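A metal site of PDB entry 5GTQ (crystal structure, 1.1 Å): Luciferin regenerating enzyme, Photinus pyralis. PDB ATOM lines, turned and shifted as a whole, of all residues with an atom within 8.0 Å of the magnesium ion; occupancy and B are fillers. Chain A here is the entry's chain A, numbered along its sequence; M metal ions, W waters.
The backbone carbonyl oxygen (O) of Asp 215 sits at hydrogen-bond distance from the backbone NH (N) of Gly 164, 2.9 Å away. The backbone NH of Asp 215 sits at hydrogen-bond distance from the backbone carbonyl oxygen of Ala 228 (2.9 Å). The side-chain amide oxygen of Asn 163 sits close to the side-chain amide nitrogen of Asn 113. The side-chain amide nitrogen of Asn 163 is in hydrogen-bond range of the side-chain hydroxyl of Ser 179 (2.7 Å). The backbone NH of Asn 163 sits at hydrogen-bond distance from the backbone carbonyl oxygen of Ile 177.
Of the 27 residues printed, 3 come within 4 Å of the magnesium ion.
The magnesium ion is bound by OE1 of Glu 21 (2.0 Å). The magnesium ion is bound by OD1 of Asp 215 (2.0 Å). Water W3 binds the magnesium ion, 2.0 Å away. The magnesium ion is bound by OD1 of Asn 163, at 2.1 Å. Water W2 is bound to the magnesium ion (2.1 Å). Water W1 is bound to the magnesium ion, at 2.2 Å.
Water W1 bridges the side-chain amide oxygen of Asn 113 (2.9 Å) and the side-chain carboxylate of Glu 21 (3.4 Å). Water W2 lies within hydrogen-bond range of the side-chain amide nitrogen (ND2) of Asn 113 (3.0 Å) and the side-chain amide nitrogen (ND2) of Asn 163 (3.2 Å). Water W3 lies within hydrogen-bond range of the side-chain carboxylate (OE2) of Glu 21, the side-chain carboxylate (OD2) of Asp 114 and the backbone NH (N) of Gly 216.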
ATOM      1  N   VAL A  19      13.062  25.913   3.298  1.00  0.00           N
ATOM      2  CA  VAL A  19      14.514  25.959   3.407  1.00  0.00           C
ATOM      3  C   VAL A  19      14.960  27.267   2.767  1.00  0.00           C
ATOM      4  O   VAL A  19      15.325  27.305   1.581  1.00  0.00           O
ATOM      5  CB  VAL A  19      15.248  24.757   2.771  1.00  0.00           C
ATOM      6  CG1 VAL A  19      16.737  24.856   3.073  1.00  0.00           C
ATOM      7  CG2 VAL A  19      14.699  23.419   3.271  1.00  0.00           C
ATOM      8  N   GLY A  20      14.882  28.364   3.520  1.00  0.00           N
ATOM      9  CA  GLY A  20      15.444  29.605   3.019  1.00  0.00           C
ATOM     10  C   GLY A  20      16.953  29.447   2.896  1.00  0.00           C
ATOM     11  O   GLY A  20      17.575  28.763   3.712  1.00  0.00           O
ATOM     12  N   GLU A  21      17.544  30.054   1.870  1.00  0.00           N
ATOM     13  CA  GLU A  21      18.922  29.718   1.514  1.00  0.00           C
ATOM     14  C   GLU A  21      19.485  30.770   0.549  1.00  0.00           C
ATOM     15  O   GLU A  21      18.768  31.640   0.043  1.00  0.00           O
ATOM     16  CB  GLU A  21      18.979  28.330   0.837  1.00  0.00           C
ATOM     17  CG  GLU A  21      19.486  27.206   1.732  1.00  0.00           C
ATOM     18  CD  GLU A  21      20.974  27.258   2.002  1.00  0.00           C
ATOM     19  OE1 GLU A  21      21.488  26.240   2.506  1.00  0.00           O
ATOM     20  OE2 GLU A  21      21.619  28.280   1.727  1.00  0.00           O
ATOM     21  N   GLY A  22      20.790  30.631   0.273  1.00  0.00           N
ATOM     22  CA  GLY A  22      21.418  31.404  -0.774  1.00  0.00           C
ATOM     23  C   GLY A  22      21.269  32.921  -0.720  1.00  0.00           C
ATOM     24  O   GLY A  22      21.040  33.557  -1.744  1.00  0.00           O
ATOM     25  N   PRO A  23      21.436  33.533   0.443  1.00  0.00           N
ATOM     26  CA  PRO A  23      21.286  35.002   0.511  1.00  0.00           C
ATOM     27  C   PRO A  23      22.401  35.719  -0.236  1.00  0.00           C
ATOM     28  O   PRO A  23      23.572  35.345  -0.162  1.00  0.00           O
ATOM     29  CB  PRO A  23      21.357  35.288   2.021  1.00  0.00           C
ATOM     30  CG  PRO A  23      22.204  34.179   2.553  1.00  0.00           C
ATOM     31  CD  PRO A  23      21.788  32.965   1.762  1.00  0.00           C
ATOM     32  N   THR A  37      15.256  26.308  -1.260  1.00  0.00           N
ATOM     33  CA  THR A  37      15.805  25.171  -2.008  1.00  0.00           C
ATOM     34  C   THR A  37      14.815  24.028  -2.201  1.00  0.00           C
ATOM     35  O   THR A  37      15.110  23.130  -2.996  1.00  0.00           O
ATOM     36  CB  THR A  37      17.085  24.641  -1.375  1.00  0.00           C
ATOM     37  OG1 THR A  37      16.828  24.329  -0.005  1.00  0.00           O
ATOM     38  CG2 THR A  37      18.228  25.634  -1.512  1.00  0.00           C
ATOM     39  N   SER A  62      18.750  26.900  -6.081  1.00  0.00           N
ATOM     40  CA  SER A  62      19.692  26.921  -4.967  1.00  0.00           C
ATOM     41  C   SER A  62      20.526  28.175  -4.842  1.00  0.00           C
ATOM     42  O   SER A  62      21.136  28.364  -3.789  1.00  0.00           O
ATOM     43  CB  SER A  62      20.596  25.682  -4.962  1.00  0.00           C
ATOM     44  OG  SER A  62      21.407  25.646  -6.121  1.00  0.00           O
ATOM     45  N   ASN A 113      23.505  22.794  -5.577  1.00  0.00           N
ATOM     46  CA  ASN A 113      23.262  23.351  -4.263  1.00  0.00           C
ATOM     47  C   ASN A 113      23.970  24.704  -4.131  1.00  0.00           C
ATOM     48  O   ASN A 113      23.775  25.565  -4.991  1.00  0.00           O
ATOM     49  CB  ASN A 113      23.534  22.356  -3.125  1.00  0.00           C
ATOM     50  CG  ASN A 113      22.886  22.805  -1.823  1.00  0.00           C
ATOM     51  OD1 ASN A 113      21.853  23.496  -1.838  1.00  0.00           O
ATOM     52  ND2 ASN A 113      23.488  22.447  -0.704  1.00  0.00           N
ATOM     53  N   ASP A 114      24.780  24.934  -3.093  1.00  0.00           N
ATOM     54  CA  ASP A 114      25.207  26.313  -2.855  1.00  0.00           C
ATOM     55  C   ASP A 114      26.128  26.795  -3.971  1.00  0.00           C
ATOM     56  O   ASP A 114      26.825  26.001  -4.629  1.00  0.00           O
ATOM     57  CB  ASP A 114      25.857  26.447  -1.475  1.00  0.00           C
ATOM     58  CG  ASP A 114      25.706  27.830  -0.860  1.00  0.00           C
ATOM     59  OD1 ASP A 114      25.088  28.743  -1.470  1.00  0.00           O
ATOM     60  OD2 ASP A 114      26.211  27.988   0.291  1.00  0.00           O
ATOM     61  N   GLY A 115      26.099  28.096  -4.196  1.00  0.00           N
ATOM     62  CA  GLY A 115      26.919  28.707  -5.235  1.00  0.00           C
ATOM     63  C   GLY A 115      27.174  30.150  -4.901  1.00  0.00           C
ATOM     64  O   GLY A 115      26.378  30.794  -4.208  1.00  0.00           O
ATOM     65  N   MET A 128      24.795  17.712  -5.472  1.00  0.00           N
ATOM     66  CA  MET A 128      24.462  16.755  -4.433  1.00  0.00           C
ATOM     67  C   MET A 128      23.342  15.877  -4.977  1.00  0.00           C
ATOM     68  O   MET A 128      22.596  16.267  -5.875  1.00  0.00           O
ATOM     69  CB  MET A 128      23.964  17.448  -3.159  1.00  0.00           C
ATOM     70  CG  MET A 128      22.688  18.241  -3.368  1.00  0.00           C
ATOM     71  SD  MET A 128      22.092  19.236  -1.987  1.00  0.00           S
ATOM     72  CE  MET A 128      21.297  18.002  -0.969  1.00  0.00           C
ATOM     73  N   ILE A 161      27.003  17.010   0.423  1.00  0.00           N
ATOM     74  CA  ILE A 161      26.096  18.153   0.353  1.00  0.00           C
ATOM     75  C   ILE A 161      26.937  19.403   0.110  1.00  0.00           C
ATOM     76  O   ILE A 161      27.521  19.967   1.041  1.00  0.00           O
ATOM     77  CB  ILE A 161      25.205  18.304   1.590  1.00  0.00           C
ATOM     78  CG1 ILE A 161      24.382  17.014   1.809  1.00  0.00           C
ATOM     79  CG2 ILE A 161      24.292  19.513   1.431  1.00  0.00           C
ATOM     80  CD1 ILE A 161      23.425  17.092   2.981  1.00  0.00           C
ATOM     81  N   ALA A 162      27.000  19.827  -1.153  1.00  0.00           N
ATOM     82  CA  ALA A 162      27.841  20.932  -1.592  1.00  0.00           C
ATOM     83  C   ALA A 162      27.331  22.229  -0.987  1.00  0.00           C
ATOM     84  O   ALA A 162      26.188  22.641  -1.252  1.00  0.00           O
ATOM     85  CB  ALA A 162      27.768  21.019  -3.111  1.00  0.00           C
ATOM     86  N   ASN A 163      28.162  22.896  -0.181  1.00  0.00           N
ATOM     87  CA  ASN A 163      27.657  24.001   0.607  1.00  0.00           C
ATOM     88  C   ASN A 163      28.569  25.225   0.561  1.00  0.00           C
ATOM     89  O   ASN A 163      29.059  25.560  -0.521  1.00  0.00           O
ATOM     90  CB  ASN A 163      27.196  23.514   1.995  1.00  0.00           C
ATOM     91  CG  ASN A 163      25.691  23.534   2.104  1.00  0.00           C
ATOM     92  OD1 ASN A 163      25.048  24.435   1.566  1.00  0.00           O
ATOM     93  ND2 ASN A 163      25.118  22.543   2.799  1.00  0.00           N
ATOM     94  N   GLY A 164      28.759  25.925   1.674  1.00  0.00           N
ATOM     95  CA  GLY A 164      29.188  27.313   1.603  1.00  0.00           C
ATOM     96  C   GLY A 164      30.605  27.503   1.066  1.00  0.00           C
ATOM     97  O   GLY A 164      31.511  26.686   1.254  1.00  0.00           O
ATOM     98  N   ILE A 177      32.729  24.038   2.197  1.00  0.00           N
ATOM     99  CA  ILE A 177      32.003  23.151   3.098  1.00  0.00           C
ATOM    100  C   ILE A 177      31.256  22.087   2.310  1.00  0.00           C
ATOM    101  O   ILE A 177      30.421  22.418   1.447  1.00  0.00           O
ATOM    102  CB  ILE A 177      30.991  23.960   3.931  1.00  0.00           C
ATOM    103  CG1 ILE A 177      31.711  24.881   4.907  1.00  0.00           C
ATOM    104  CG2 ILE A 177      30.014  23.043   4.650  1.00  0.00           C
ATOM    105  CD1 ILE A 177      30.840  26.023   5.421  1.00  0.00           C
ATOM    106  N   SER A 179      28.658  19.626   3.920  1.00  0.00           N
ATOM    107  CA  SER A 179      28.066  19.468   5.256  1.00  0.00           C
ATOM    108  C   SER A 179      28.335  18.090   5.848  1.00  0.00           C
ATOM    109  O   SER A 179      28.477  17.960   7.070  1.00  0.00           O
ATOM    110  CB  SER A 179      26.559  19.671   5.197  1.00  0.00           C
ATOM    111  OG  SER A 179      26.249  20.971   4.746  1.00  0.00           O
ATOM    112  N   PRO A 214      27.906  22.298   9.303  1.00  0.00           N
ATOM    113  CA  PRO A 214      28.155  23.560   8.601  1.00  0.00           C
ATOM    114  C   PRO A 214      27.351  23.581   7.322  1.00  0.00           C
ATOM    115  O   PRO A 214      27.206  22.547   6.655  1.00  0.00           O
ATOM    116  CB  PRO A 214      29.659  23.505   8.321  1.00  0.00           C
ATOM    117  CG  PRO A 214      29.979  22.022   8.196  1.00  0.00           C
ATOM    118  CD  PRO A 214      29.038  21.338   9.169  1.00  0.00           C
ATOM    119  N   ASP A 215      26.840  24.763   6.963  1.00  0.00           N
ATOM    120  CA  ASP A 215      25.977  24.912   5.790  1.00  0.00           C
ATOM    121  C   ASP A 215      26.554  26.024   4.926  1.00  0.00           C
ATOM    122  O   ASP A 215      27.635  25.838   4.361  1.00  0.00           O
ATOM    123  CB  ASP A 215      24.515  25.070   6.262  1.00  0.00           C
ATOM    124  CG  ASP A 215      23.479  24.786   5.196  1.00  0.00           C
ATOM    125  OD1 ASP A 215      23.779  24.957   3.988  1.00  0.00           O
ATOM    126  OD2 ASP A 215      22.354  24.383   5.587  1.00  0.00           O
ATOM    127  N   GLY A 216      25.892  27.187   4.835  1.00  0.00           N
ATOM    128  CA  GLY A 216      26.484  28.318   4.131  1.00  0.00           C
ATOM    129  C   GLY A 216      27.542  29.000   4.977  1.00  0.00           C
ATOM    130  O   GLY A 216      27.617  28.829   6.192  1.00  0.00           O
ATOM    131  N   GLN A 217      28.374  29.825   4.333  1.00  0.00           N
ATOM    132  CA  GLN A 217      29.340  30.627   5.069  1.00  0.00           C
ATOM    133  C   GLN A 217      29.651  31.907   4.310  1.00  0.00           C
ATOM    134  O   GLN A 217      29.401  32.020   3.101  1.00  0.00           O
ATOM    135  CB  GLN A 217      30.649  29.876   5.360  1.00  0.00           C
ATOM    136  CG  GLN A 217      31.478  29.551   4.124  1.00  0.00           C
ATOM    137  CD  GLN A 217      32.752  28.790   4.436  1.00  0.00           C
ATOM    138  OE1 GLN A 217      33.308  28.934   5.523  1.00  0.00           O
ATOM    139  NE2 GLN A 217      33.242  28.005   3.468  1.00  0.00           N
ATOM    140  N   ALA A 228      27.061  29.171   9.039  1.00  0.00           N
ATOM    141  CA  ALA A 228      25.745  28.743   9.477  1.00  0.00           C
ATOM    142  C   ALA A 228      25.811  27.317   9.993  1.00  0.00           C
ATOM    143  O   ALA A 228      26.415  26.441   9.351  1.00  0.00           O
ATOM    144  CB  ALA A 228      24.773  28.787   8.298  1.00  0.00           C
ATOM    145  N   PHE A 230      23.512  24.302  10.710  1.00  0.00           N
ATOM    146  CA  PHE A 230      22.217  23.661  10.539  1.00  0.00           C
ATOM    147  C   PHE A 230      22.063  22.593  11.623  1.00  0.00           C
ATOM    148  O   PHE A 230      22.937  21.733  11.775  1.00  0.00           O
ATOM    149  CB  PHE A 230      22.188  23.005   9.145  1.00  0.00           C
ATOM    150  CG  PHE A 230      20.823  22.487   8.749  1.00  0.00           C
ATOM    151  CD1 PHE A 230      19.981  23.275   7.974  1.00  0.00           C
ATOM    152  CD2 PHE A 230      20.388  21.229   9.141  1.00  0.00           C
ATOM    153  CE1 PHE A 230      18.736  22.832   7.599  1.00  0.00           C
ATOM    154  CE2 PHE A 230      19.122  20.768   8.761  1.00  0.00           C
ATOM    155  CZ  PHE A 230      18.310  21.573   7.995  1.00  0.00           C
ATOM    156  N   VAL A 257      19.738  26.808  11.008  1.00  0.00           N
ATOM    157  CA  VAL A 257      20.383  27.950  10.358  1.00  0.00           C
ATOM    158  C   VAL A 257      21.035  27.454   9.083  1.00  0.00           C
ATOM    159  O   VAL A 257      21.759  26.450   9.098  1.00  0.00           O
ATOM    160  CB  VAL A 257      21.417  28.576  11.312  1.00  0.00           C
ATOM    161  CG1 VAL A 257      22.071  29.766  10.652  1.00  0.00           C
ATOM    162  CG2 VAL A 257      20.752  28.987  12.618  1.00  0.00           C
ATOM    163  N   THR A 258      20.789  28.147   7.966  1.00  0.00           N
ATOM    164  CA  THR A 258      21.212  27.648   6.658  1.00  0.00           C
ATOM    165  C   THR A 258      22.329  28.460   6.020  1.00  0.00           C
ATOM    166  O   THR A 258      23.223  27.867   5.412  1.00  0.00           O
ATOM    167  CB  THR A 258      20.036  27.543   5.670  1.00  0.00           C
ATOM    168  OG1 THR A 258      19.446  28.832   5.551  1.00  0.00           O
ATOM    169  CG2 THR A 258      18.994  26.550   6.157  1.00  0.00           C
ATOM    170  N   SER A 259      22.274  29.792   6.069  1.00  0.00           N
ATOM    171  CA  SER A 259      23.293  30.570   5.374  1.00  0.00           C
ATOM    172  C   SER A 259      23.304  31.994   5.890  1.00  0.00           C
ATOM    173  O   SER A 259      22.515  32.363   6.768  1.00  0.00           O
ATOM    174  CB  SER A 259      23.135  30.487   3.857  1.00  0.00           C
ATOM    175  OG  SER A 259      24.321  30.938   3.253  1.00  0.00           O
ATOM    176  N   THR A 273      19.590  33.157   6.995  1.00  0.00           N
ATOM    177  CA  THR A 273      18.443  32.362   6.573  1.00  0.00           C
ATOM    178  C   THR A 273      18.334  31.103   7.426  1.00  0.00           C
ATOM    179  O   THR A 273      19.306  30.653   8.046  1.00  0.00           O
ATOM    180  CB  THR A 273      18.549  32.001   5.072  1.00  0.00           C
ATOM    181  OG1 THR A 273      19.851  31.465   4.787  1.00  0.00           O
ATOM    182  CG2 THR A 273      18.349  33.225   4.206  1.00  0.00           C
HETATM  183 MG    MG M   1      23.251  25.374   2.069  1.00  0.00          MG
HETATM  184  O   HOH W   1      22.746  25.598  -0.010  1.00  0.00           O
HETATM  185  O   HOH W   2      22.212  23.523   1.778  1.00  0.00           O
HETATM  186  O   HOH W   3      24.103  27.230   2.003  1.00  0.00           O
